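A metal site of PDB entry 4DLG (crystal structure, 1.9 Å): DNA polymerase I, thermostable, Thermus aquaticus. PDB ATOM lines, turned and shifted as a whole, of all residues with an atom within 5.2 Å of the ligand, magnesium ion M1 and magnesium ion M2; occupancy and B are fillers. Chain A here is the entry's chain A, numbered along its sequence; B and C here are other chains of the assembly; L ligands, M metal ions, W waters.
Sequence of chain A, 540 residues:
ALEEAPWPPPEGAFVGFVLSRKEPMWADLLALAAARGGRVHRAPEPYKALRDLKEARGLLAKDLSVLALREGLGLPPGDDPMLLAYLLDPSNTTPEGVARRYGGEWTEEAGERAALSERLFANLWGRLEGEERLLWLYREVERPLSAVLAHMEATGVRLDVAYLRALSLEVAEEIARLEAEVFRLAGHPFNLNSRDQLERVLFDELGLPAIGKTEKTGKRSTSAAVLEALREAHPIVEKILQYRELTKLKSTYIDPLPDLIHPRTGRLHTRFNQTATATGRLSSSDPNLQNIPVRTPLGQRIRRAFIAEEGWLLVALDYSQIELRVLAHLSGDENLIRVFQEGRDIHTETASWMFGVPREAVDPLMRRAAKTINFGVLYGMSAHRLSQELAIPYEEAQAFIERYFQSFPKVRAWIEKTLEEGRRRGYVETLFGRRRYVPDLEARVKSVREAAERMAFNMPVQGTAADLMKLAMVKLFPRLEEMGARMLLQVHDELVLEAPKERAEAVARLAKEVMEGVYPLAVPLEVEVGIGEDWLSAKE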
ATOM      1  N   ARG A 281      22.705   4.510   8.976  1.00  0.00           N
ATOM      2  CA  ARG A 281      21.532   5.353   8.845  1.00  0.00           C
ATOM      3  C   ARG A 281      21.859   6.789   9.247  1.00  0.00           C
ATOM      4  O   ARG A 281      22.845   7.048   9.931  1.00  0.00           O
ATOM      5  CB  ARG A 281      20.391   4.848   9.729  1.00  0.00           C
ATOM      6  CG  ARG A 281      19.457   3.844   9.056  1.00  0.00           C
ATOM      7  CD  ARG A 281      18.211   3.643   9.914  1.00  0.00           C
ATOM      8  NE  ARG A 281      17.226   2.784   9.269  1.00  0.00           N
ATOM      9  CZ  ARG A 281      16.013   2.547   9.762  1.00  0.00           C
ATOM     10  NH1 ARG A 281      15.639   3.113  10.897  1.00  0.00           N
ATOM     11  NH2 ARG A 281      15.174   1.748   9.112  1.00  0.00           N
ATOM     12  N   ASP A 318       8.292   6.854  -0.970  1.00  0.00           N
ATOM     13  CA  ASP A 318       8.673   5.811  -0.022  1.00  0.00           C
ATOM     14  C   ASP A 318       9.012   4.511  -0.741  1.00  0.00           C
ATOM     15  O   ASP A 318       8.247   4.035  -1.582  1.00  0.00           O
ATOM     16  CB  ASP A 318       7.549   5.584   0.998  1.00  0.00           C
ATOM     17  CG  ASP A 318       7.974   4.713   2.168  1.00  0.00           C
ATOM     18  OD1 ASP A 318       8.741   3.759   1.965  1.00  0.00           O
ATOM     19  OD2 ASP A 318       7.527   4.985   3.308  1.00  0.00           O
ATOM     20  N   TYR A 319      10.157   3.935  -0.394  1.00  0.00           N
ATOM     21  CA  TYR A 319      10.547   2.616  -0.908  1.00  0.00           C
ATOM     22  C   TYR A 319       9.588   1.556  -0.378  1.00  0.00           C
ATOM     23  O   TYR A 319       9.238   1.552   0.800  1.00  0.00           O
ATOM     24  CB  TYR A 319      11.968   2.267  -0.494  1.00  0.00           C
ATOM     25  CG  TYR A 319      13.053   2.840  -1.374  1.00  0.00           C
ATOM     26  CD1 TYR A 319      13.278   2.339  -2.656  1.00  0.00           C
ATOM     27  CD2 TYR A 319      13.860   3.880  -0.937  1.00  0.00           C
ATOM     28  CE1 TYR A 319      14.266   2.864  -3.466  1.00  0.00           C
ATOM     29  CE2 TYR A 319      14.858   4.409  -1.733  1.00  0.00           C
ATOM     30  CZ  TYR A 319      15.051   3.893  -3.002  1.00  0.00           C
ATOM     31  OH  TYR A 319      16.039   4.414  -3.803  1.00  0.00           O
ATOM     32  N   SER A 320       9.182   0.646  -1.254  1.00  0.00           N
ATOM     33  CA  SER A 320       8.258  -0.432  -0.883  1.00  0.00           C
ATOM     34  C   SER A 320       8.995  -1.696  -0.468  1.00  0.00           C
ATOM     35  O   SER A 320       9.724  -2.285  -1.257  1.00  0.00           O
ATOM     36  CB  SER A 320       7.318  -0.741  -2.048  1.00  0.00           C
ATOM     37  OG  SER A 320       6.889  -2.093  -2.014  1.00  0.00           O
ATOM     38  N   GLN A 321       8.790  -2.113   0.779  1.00  0.00           N
ATOM     39  CA  GLN A 321       9.405  -3.321   1.330  1.00  0.00           C
ATOM     40  C   GLN A 321      10.917  -3.347   1.138  1.00  0.00           C
ATOM     41  O   GLN A 321      11.484  -4.368   0.770  1.00  0.00           O
ATOM     42  CB  GLN A 321       8.759  -4.573   0.733  1.00  0.00           C
ATOM     43  CG  GLN A 321       7.263  -4.698   0.991  1.00  0.00           C
ATOM     44  CD  GLN A 321       6.457  -4.776  -0.290  1.00  0.00           C
ATOM     45  OE1 GLN A 321       6.006  -3.760  -0.827  1.00  0.00           O
ATOM     46  NE2 GLN A 321       6.261  -5.989  -0.791  1.00  0.00           N
ATOM     47  N   ILE A 322      11.558  -2.207   1.399  1.00  0.00           N
ATOM     48  CA  ILE A 322      12.971  -2.014   1.099  1.00  0.00           C
ATOM     49  C   ILE A 322      13.907  -3.055   1.727  1.00  0.00           C
ATOM     50  O   ILE A 322      14.743  -3.640   1.036  1.00  0.00           O
ATOM     51  CB  ILE A 322      13.442  -0.569   1.438  1.00  0.00           C
ATOM     52  CG1 ILE A 322      14.941  -0.409   1.175  1.00  0.00           C
ATOM     53  CG2 ILE A 322      13.081  -0.190   2.864  1.00  0.00           C
ATOM     54  CD1 ILE A 322      15.331  -0.567  -0.282  1.00  0.00           C
ATOM     55  N   GLU A 323      13.753  -3.313   3.027  1.00  0.00           N
ATOM     56  CA  GLU A 323      14.644  -4.264   3.703  1.00  0.00           C
ATOM     57  C   GLU A 323      14.344  -5.714   3.352  1.00  0.00           C
ATOM     58  O   GLU A 323      15.225  -6.584   3.459  1.00  0.00           O
ATOM     59  CB  GLU A 323      14.608  -4.055   5.220  1.00  0.00           C
ATOM     60  CG  GLU A 323      15.311  -2.786   5.674  1.00  0.00           C
ATOM     61  CD  GLU A 323      15.553  -2.749   7.169  1.00  0.00           C
ATOM     62  OE1 GLU A 323      15.235  -3.751   7.851  1.00  0.00           O
ATOM     63  OE2 GLU A 323      16.045  -1.718   7.667  1.00  0.00           O
ATOM     64  N   HIS A 347       3.682  -7.579   3.450  1.00  0.00           N
ATOM     65  CA  HIS A 347       2.999  -6.796   4.461  1.00  0.00           C
ATOM     66  C   HIS A 347       1.485  -6.942   4.378  1.00  0.00           C
ATOM     67  O   HIS A 347       0.788  -6.971   5.388  1.00  0.00           O
ATOM     68  CB  HIS A 347       3.381  -5.318   4.347  1.00  0.00           C
ATOM     69  CG  HIS A 347       4.814  -5.033   4.694  1.00  0.00           C
ATOM     70  ND1 HIS A 347       5.620  -5.947   5.325  1.00  0.00           N
ATOM     71  CD2 HIS A 347       5.582  -3.936   4.473  1.00  0.00           C
ATOM     72  CE1 HIS A 347       6.818  -5.430   5.504  1.00  0.00           C
ATOM     73  NE2 HIS A 347       6.824  -4.212   4.994  1.00  0.00           N
ATOM     74  N   ARG A 367      -2.287  -2.897   7.385  1.00  0.00           N
ATOM     75  CA  ARG A 367      -1.040  -3.227   6.708  1.00  0.00           C
ATOM     76  C   ARG A 367       0.186  -2.781   7.506  1.00  0.00           C
ATOM     77  O   ARG A 367       1.170  -3.503   7.588  1.00  0.00           O
ATOM     78  CB  ARG A 367      -1.015  -2.618   5.303  1.00  0.00           C
ATOM     79  CG  ARG A 367       0.225  -2.988   4.497  1.00  0.00           C
ATOM     80  CD  ARG A 367       0.235  -2.294   3.150  1.00  0.00           C
ATOM     81  NE  ARG A 367       1.424  -2.642   2.372  1.00  0.00           N
ATOM     82  CZ  ARG A 367       2.585  -2.004   2.460  1.00  0.00           C
ATOM     83  NH1 ARG A 367       2.721  -0.984   3.298  1.00  0.00           N
ATOM     84  NH2 ARG A 367       3.609  -2.390   1.719  1.00  0.00           N
ATOM     85  N   LYS A 371       3.804  -4.677   9.648  1.00  0.00           N
ATOM     86  CA  LYS A 371       5.212  -4.352   9.472  1.00  0.00           C
ATOM     87  C   LYS A 371       6.033  -4.764  10.691  1.00  0.00           C
ATOM     88  O   LYS A 371       7.107  -5.340  10.560  1.00  0.00           O
ATOM     89  CB  LYS A 371       5.401  -2.852   9.212  1.00  0.00           C
ATOM     90  CG  LYS A 371       4.780  -2.365   7.922  1.00  0.00           C
ATOM     91  CD  LYS A 371       5.096  -0.896   7.690  1.00  0.00           C
ATOM     92  CE  LYS A 371       4.516  -0.395   6.387  1.00  0.00           C
ATOM     93  NZ  LYS A 371       4.880   1.029   6.127  1.00  0.00           N
ATOM     94  N   THR A 372       5.504  -4.475  11.876  1.00  0.00           N
ATOM     95  CA  THR A 372       6.147  -4.835  13.126  1.00  0.00           C
ATOM     96  C   THR A 372       6.285  -6.350  13.229  1.00  0.00           C
ATOM     97  O   THR A 372       7.222  -6.877  13.835  1.00  0.00           O
ATOM     98  CB  THR A 372       5.355  -4.313  14.341  1.00  0.00           C
ATOM     99  OG1 THR A 372       5.140  -2.905  14.195  1.00  0.00           O
ATOM    100  CG2 THR A 372       6.114  -4.572  15.644  1.00  0.00           C
ATOM    101  N   PHE A 375       8.953  -7.611  10.161  1.00  0.00           N
ATOM    102  CA  PHE A 375      10.306  -7.202  10.512  1.00  0.00           C
ATOM    103  C   PHE A 375      10.707  -7.771  11.870  1.00  0.00           C
ATOM    104  O   PHE A 375      11.865  -8.130  12.073  1.00  0.00           O
ATOM    105  CB  PHE A 375      10.416  -5.675  10.521  1.00  0.00           C
ATOM    106  CG  PHE A 375      10.149  -5.048   9.189  1.00  0.00           C
ATOM    107  CD1 PHE A 375      10.611  -5.649   8.023  1.00  0.00           C
ATOM    108  CD2 PHE A 375       9.443  -3.859   9.083  1.00  0.00           C
ATOM    109  CE1 PHE A 375      10.376  -5.079   6.788  1.00  0.00           C
ATOM    110  CE2 PHE A 375       9.197  -3.293   7.857  1.00  0.00           C
ATOM    111  CZ  PHE A 375       9.669  -3.899   6.701  1.00  0.00           C
ATOM    112  N   TYR A 379      13.970 -10.500  12.494  1.00  0.00           N
ATOM    113  CA  TYR A 379      15.164 -10.217  13.293  1.00  0.00           C
ATOM    114  C   TYR A 379      15.108 -10.833  14.693  1.00  0.00           C
ATOM    115  O   TYR A 379      15.538 -10.213  15.672  1.00  0.00           O
ATOM    116  CB  TYR A 379      15.420  -8.712  13.380  1.00  0.00           C
ATOM    117  CG  TYR A 379      15.567  -8.056  12.026  1.00  0.00           C
ATOM    118  CD1 TYR A 379      16.631  -8.369  11.189  1.00  0.00           C
ATOM    119  CD2 TYR A 379      14.656  -7.112  11.587  1.00  0.00           C
ATOM    120  CE1 TYR A 379      16.780  -7.776   9.950  1.00  0.00           C
ATOM    121  CE2 TYR A 379      14.785  -6.499  10.356  1.00  0.00           C
ATOM    122  CZ  TYR A 379      15.847  -6.834   9.542  1.00  0.00           C
ATOM    123  OH  TYR A 379      15.985  -6.235   8.315  1.00  0.00           O
ATOM    124  N   VAL A 491      13.509  10.309   5.688  1.00  0.00           N
ATOM    125  CA  VAL A 491      13.065   9.451   6.775  1.00  0.00           C
ATOM    126  C   VAL A 491      13.444   7.994   6.495  1.00  0.00           C
ATOM    127  O   VAL A 491      12.576   7.155   6.231  1.00  0.00           O
ATOM    128  CB  VAL A 491      11.547   9.560   7.026  1.00  0.00           C
ATOM    129  CG1 VAL A 491      11.196   9.016   8.403  1.00  0.00           C
ATOM    130  CG2 VAL A 491      11.104  11.014   6.905  1.00  0.00           C
ATOM    131  N   ASP A 493      13.797   5.501   4.643  1.00  0.00           N
ATOM    132  CA  ASP A 493      13.463   5.019   3.294  1.00  0.00           C
ATOM    133  C   ASP A 493      12.481   5.959   2.606  1.00  0.00           C
ATOM    134  O   ASP A 493      11.820   5.591   1.634  1.00  0.00           O
ATOM    135  CB  ASP A 493      12.927   3.582   3.337  1.00  0.00           C
ATOM    136  CG  ASP A 493      11.458   3.501   3.737  1.00  0.00           C
ATOM    137  OD1 ASP A 493      10.981   4.353   4.519  1.00  0.00           O
ATOM    138  OD2 ASP A 493      10.790   2.548   3.283  1.00  0.00           O
ATOM    139  N   GLU A 494      12.397   7.190   3.104  1.00  0.00           N
ATOM    140  CA  GLU A 494      11.440   8.161   2.586  1.00  0.00           C
ATOM    141  C   GLU A 494      12.091   9.516   2.296  1.00  0.00           C
ATOM    142  O   GLU A 494      12.969   9.965   3.035  1.00  0.00           O
ATOM    143  CB  GLU A 494      10.279   8.344   3.578  1.00  0.00           C
ATOM    144  CG  GLU A 494       9.210   9.309   3.114  1.00  0.00           C
ATOM    145  CD  GLU A 494       8.130   9.524   4.148  1.00  0.00           C
ATOM    146  OE1 GLU A 494       8.099   8.768   5.148  1.00  0.00           O
ATOM    147  OE2 GLU A 494       7.306  10.445   3.969  1.00  0.00           O
ATOM    148  N   LYS A 539       0.959  11.423   1.274  1.00  0.00           N
ATOM    149  CA  LYS A 539       1.143   9.975   1.345  1.00  0.00           C
ATOM    150  C   LYS A 539      -0.207   9.256   1.317  1.00  0.00           C
ATOM    151  O   LYS A 539      -0.414   8.283   2.041  1.00  0.00           O
ATOM    152  CB  LYS A 539       1.924   9.586   2.593  1.00  0.00           C
ATOM    153  CG  LYS A 539       3.306  10.228   2.688  1.00  0.00           C
ATOM    154  CD  LYS A 539       4.182   9.513   3.698  1.00  0.00           C
ATOM    155  CE  LYS A 539       4.459   8.085   3.270  1.00  0.00           C
ATOM    156  NZ  LYS A 539       5.326   7.364   4.244  1.00  0.00           N
ATOM    157  P    DG B   4      11.890 -10.164  21.660  1.00  0.00           P
ATOM    158  OP1  DG B   4      10.557 -10.507  22.184  1.00  0.00           O
ATOM    159  OP2  DG B   4      12.835 -11.243  21.295  1.00  0.00           O
ATOM    160  O5'  DG B   4      11.715  -9.242  20.367  1.00  0.00           O
ATOM    161  C5'  DG B   4      12.661  -8.197  20.115  1.00  0.00           C
ATOM    162  C4'  DG B   4      13.494  -8.471  18.882  1.00  0.00           C
ATOM    163  O4'  DG B   4      12.615  -8.748  17.759  1.00  0.00           O
ATOM    164  C3'  DG B   4      14.386  -7.312  18.458  1.00  0.00           C
ATOM    165  O3'  DG B   4      15.693  -7.522  18.969  1.00  0.00           O
ATOM    166  C2'  DG B   4      14.371  -7.405  16.934  1.00  0.00           C
ATOM    167  C1'  DG B   4      12.965  -7.941  16.653  1.00  0.00           C
ATOM    168  N9   DG B   4      11.948  -6.904  16.511  1.00  0.00           N
ATOM    169  C8   DG B   4      10.867  -6.690  17.325  1.00  0.00           C
ATOM    170  N7   DG B   4      10.119  -5.684  16.947  1.00  0.00           N
ATOM    171  C5   DG B   4      10.756  -5.207  15.804  1.00  0.00           C
ATOM    172  C6   DG B   4      10.404  -4.127  14.963  1.00  0.00           C
ATOM    173  O6   DG B   4       9.436  -3.363  15.054  1.00  0.00           O
ATOM    174  N1   DG B   4      11.312  -3.973  13.916  1.00  0.00           N
ATOM    175  C2   DG B   4      12.423  -4.771  13.711  1.00  0.00           C
ATOM    176  N2   DG B   4      13.183  -4.472  12.652  1.00  0.00           N
ATOM    177  N3   DG B   4      12.762  -5.785  14.503  1.00  0.00           N
ATOM    178  C4   DG B   4      11.884  -5.947  15.516  1.00  0.00           C
ATOM    179  P    DG B   5      16.493  -6.309  19.658  1.00  0.00           P
ATOM    180  OP1  DG B   5      17.632  -6.878  20.403  1.00  0.00           O
ATOM    181  OP2  DG B   5      15.507  -5.456  20.358  1.00  0.00           O
ATOM    182  O5'  DG B   5      17.052  -5.467  18.419  1.00  0.00           O
ATOM    183  C5'  DG B   5      18.048  -6.027  17.555  1.00  0.00           C
ATOM    184  C4'  DG B   5      18.226  -5.189  16.306  1.00  0.00           C
ATOM    185  O4'  DG B   5      16.992  -5.189  15.542  1.00  0.00           O
ATOM    186  C3'  DG B   5      18.532  -3.713  16.548  1.00  0.00           C
ATOM    187  O3'  DG B   5      19.937  -3.529  16.683  1.00  0.00           O
ATOM    188  C2'  DG B   5      18.024  -3.065  15.273  1.00  0.00           C
ATOM    189  C1'  DG B   5      16.805  -3.933  14.925  1.00  0.00           C
ATOM    190  N9   DG B   5      15.547  -3.356  15.371  1.00  0.00           N
ATOM    191  C8   DG B   5      14.769  -3.753  16.430  1.00  0.00           C
ATOM    192  N7   DG B   5      13.695  -3.036  16.590  1.00  0.00           N
ATOM    193  C5   DG B   5      13.750  -2.104  15.561  1.00  0.00           C
ATOM    194  C6   DG B   5      12.863  -1.059  15.213  1.00  0.00           C
ATOM    195  O6   DG B   5      11.801  -0.749  15.764  1.00  0.00           O
ATOM    196  N1   DG B   5      13.296  -0.353  14.101  1.00  0.00           N
ATOM    197  C2   DG B   5      14.459  -0.614  13.404  1.00  0.00           C
ATOM    198  N2   DG B   5      14.725   0.179  12.362  1.00  0.00           N
ATOM    199  N3   DG B   5      15.303  -1.585  13.716  1.00  0.00           N
ATOM    200  C4   DG B   5      14.892  -2.289  14.798  1.00  0.00           C
ATOM    201  N1  DOC C  12      11.066   3.143  11.318  1.00  0.00           N
ATOM    202  C2  DOC C  12      11.955   2.266  11.950  1.00  0.00           C
ATOM    203  N3  DOC C  12      11.541   1.521  13.002  1.00  0.00           N
ATOM    204  C4  DOC C  12      10.265   1.610  13.438  1.00  0.00           C
ATOM    205  C5  DOC C  12       9.374   2.469  12.820  1.00  0.00           C
ATOM    206  C6  DOC C  12       9.801   3.230  11.732  1.00  0.00           C
ATOM    207  O2  DOC C  12      13.139   2.177  11.551  1.00  0.00           O
ATOM    208  N4  DOC C  12       9.862   0.864  14.490  1.00  0.00           N
ATOM    209  C1' DOC C  12      11.508   3.949  10.175  1.00  0.00           C
ATOM    210  C2' DOC C  12      11.164   3.228   8.872  1.00  0.00           C
ATOM    211  C3' DOC C  12      10.245   4.164   8.110  1.00  0.00           C
ATOM    212  C4' DOC C  12      10.318   5.482   8.857  1.00  0.00           C
ATOM    213  O4' DOC C  12      10.812   5.190  10.170  1.00  0.00           O
ATOM    214  C5' DOC C  12       8.939   6.121   8.938  1.00  0.00           C
ATOM    215  O5' DOC C  12       8.049   5.251   9.623  1.00  0.00           O
ATOM    216  P   DOC C  12       6.547   5.745   9.970  1.00  0.00           P
ATOM    217  OP1 DOC C  12       5.798   4.601  10.610  1.00  0.00           O
ATOM    218  OP2 DOC C  12       5.999   6.421   8.737  1.00  0.00           O
HETATM  219  N1  LIG L   1      11.539  -1.007   9.713  1.00  0.00           N
HETATM  220  C1  LIG L   1      11.824  -1.770  10.833  1.00  0.00           C
HETATM  221  N2  LIG L   1      10.855  -1.967  11.790  1.00  0.00           N
HETATM  222  C2  LIG L   1       9.601  -1.406  11.637  1.00  0.00           C
HETATM  223  C3  LIG L   1       9.326  -0.649  10.505  1.00  0.00           C
HETATM  224  C4  LIG L   1      10.304  -0.452   9.548  1.00  0.00           C
HETATM  225  O1  LIG L   1      12.934  -2.262  10.973  1.00  0.00           O
HETATM  226  N3  LIG L   1       8.664  -1.598  12.555  1.00  0.00           N
HETATM  227  C5  LIG L   1      12.582  -0.796   8.691  1.00  0.00           C
HETATM  228  C6  LIG L   1      12.336  -1.736   7.518  1.00  0.00           C
HETATM  229  C7  LIG L   1      12.165  -0.847   6.298  1.00  0.00           C
HETATM  230  C8  LIG L   1      12.446   0.565   6.784  1.00  0.00           C
HETATM  231  O2  LIG L   1      12.506   0.532   8.190  1.00  0.00           O
HETATM  232  C9  LIG L   1      11.356   1.508   6.298  1.00  0.00           C
HETATM  233  O3  LIG L   1      10.143   1.238   6.963  1.00  0.00           O
HETATM  234  P1  LIG L   1       8.746   1.187   6.164  1.00  0.00           P
HETATM  235  O4  LIG L   1       7.630   1.637   7.070  1.00  0.00           O
HETATM  236  O5  LIG L   1       8.784   2.026   4.906  1.00  0.00           O
HETATM  237  O6  LIG L   1       8.558  -0.366   5.809  1.00  0.00           O
HETATM  238  P2  LIG L   1       8.400  -0.883   4.293  1.00  0.00           P
HETATM  239  O7  LIG L   1       8.852  -2.318   4.226  1.00  0.00           O
HETATM  240  O8  LIG L   1       9.180  -0.024   3.331  1.00  0.00           O
HETATM  241  O9  LIG L   1       6.822  -0.803   4.011  1.00  0.00           O
HETATM  242  P3  LIG L   1       6.190   0.144   2.870  1.00  0.00           P
HETATM  243  O10 LIG L   1       6.007  -0.678   1.622  1.00  0.00           O
HETATM  244  O11 LIG L   1       7.116   1.302   2.590  1.00  0.00           O
HETATM  245  O12 LIG L   1       4.847   0.660   3.316  1.00  0.00           O
HETATM  246 MG    MG M   1       8.927   1.901   2.677  1.00  0.00          MG
HETATM  247 MG    MG M   2       8.854   4.304   4.862  1.00  0.00          MG
HETATM  248  O   HOH W   1       6.122   2.402   0.326  1.00  0.00           O
HETATM  249  O   HOH W   2       6.515   1.802   9.582  1.00  0.00           O
HETATM  250  O   HOH W   3       5.457   3.552   4.497  1.00  0.00           O
HETATM  251  O   HOH W   4       7.247   4.469   6.173  1.00  0.00           O
HETATM  252  O   HOH W   5      16.054  -2.550  10.490  1.00  0.00           O
HETATM  253  O   HOH W   6       6.477  -0.151  12.122  1.00  0.00           O
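O1 of the ligand sits close to N2 of DG 5 of chain B (3.3 Å). CA of Ser 320 touches O10 of the ligand, 3.4 Å away. CG2 of Ile 322 touches C7 of the ligand, 3.6 Å away. CD of Glu 323 touches C6 of the ligand, 3.4 Å away. Phe 375 touches the ligand. Hydrophobic or aromatic side chains within 4 Å of the ligand: Ile 322, His 347 and Phe 375. Within 4 Å of the ligand: Arg 281, Asp 318, Tyr 319, Ser 320, Gln 321, Ile 322, Glu 323, His 347, Arg 367, Lys 371, Phe 375, Asp 493, DG 4 of chain B, DG 5 of chain B and DOC 12 of chain C.
Of the 20 residues printed, 3 come within 4 Å of magnesium ion M1.
Water W4 binds magnesium ion M2 (2.1 Å). Magnesium ion M2 is bound by OD1 of Asp 493 (2.2 Å). OD2 of Asp 318 is bound to magnesium ion M2, at 2.2 Å. O5 of the ligand binds magnesium ion M2 (2.3 Å).
N4 of DOC 12 of chain C lies within hydrogen-bond range of a nitrogen (N3) of the ligand, at 3.4 Å. A ring nitrogen (NE2) of His 347 is in hydrogen-bond range of an oxygen (O7) of the ligand (2.9 Å). An oxygen (O12) of the ligand lies within salt-bridge range of the side-chain amino group (NZ) of Lys 371 (2.8 Å). O6 of DG 4 of chain B is in hydrogen-bond range of a nitrogen (N3) of the ligand (3.2 Å). The guanidinium group of Arg 281 sits at hydrogen-bond distance from an oxygen (O2) of the ligand, 3.1 Å away. The guanidinium group (NH1) of Arg 367 is in salt-bridge range of an oxygen (O12) of the ligand (2.7 Å). An oxygen (O10) of the ligand is in hydrogen-bond range of the backbone NH (N) of Gln 321, at 3.2 Å.
DOC 12 of chain C touches magnesium ion M2 (C3' to MG, 3.5 Å). Within 4 Å of magnesium ion M2: Asp 318, Asp 493 and DOC 12 of chain C. Along chain A the residues within 4 Å of magnesium ion M2 span positions 318 to 493.
OH of Tyr 379 sits at hydrogen-bond distance from OE1 of Glu 323, 2.6 Å away. NH2 of Arg 281 lies within salt-bridge range of OE2 of Glu 323 (3.9 Å). NH1 of Arg 281 sits at hydrogen-bond distance from N2 of DG 5 of chain B, 3.4 Å away. O2 of DOC 12 of chain C is in hydrogen-bond range of the guanidinium group (NH1) of Arg 281. N2 of DG 5 of chain B lies close to O2 of DOC 12 of chain C (2.7 Å). NZ of Lys 539 lies close to OD2 of Asp 318.
An oxygen (O11) of the ligand binds magnesium ion M1 (1.9 Å). Magnesium ion M1 is bound by O of Tyr 319, at 1.9 Å. Magnesium ion M1 is bound by OD1 of Asp 318, at 2.0 Å. O8 of the ligand is bound to magnesium ion M1 (2.0 Å). OD2 of Asp 493 binds magnesium ion M1, 2.1 Å away. O5 of the ligand is bound to magnesium ion M1 (2.2 Å).
Water W4 lies within hydrogen-bond range of an oxygen (O4) of the ligand (3.0 Å) and OP2 of DOC 12 of chain C (3.5 Å). Water W1 bridges the backbone carbonyl oxygen of Asp 318 (3.3 Å) and an oxygen (O10) of the ligand (3.3 Å). Water W2 bridges O4 of the ligand (2.8 Å) and OP1 of DOC 12 of chain C (3.1 Å). Water W3 bridges the side-chain amino group of Lys 371 and an oxygen (O12) of the ligand.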
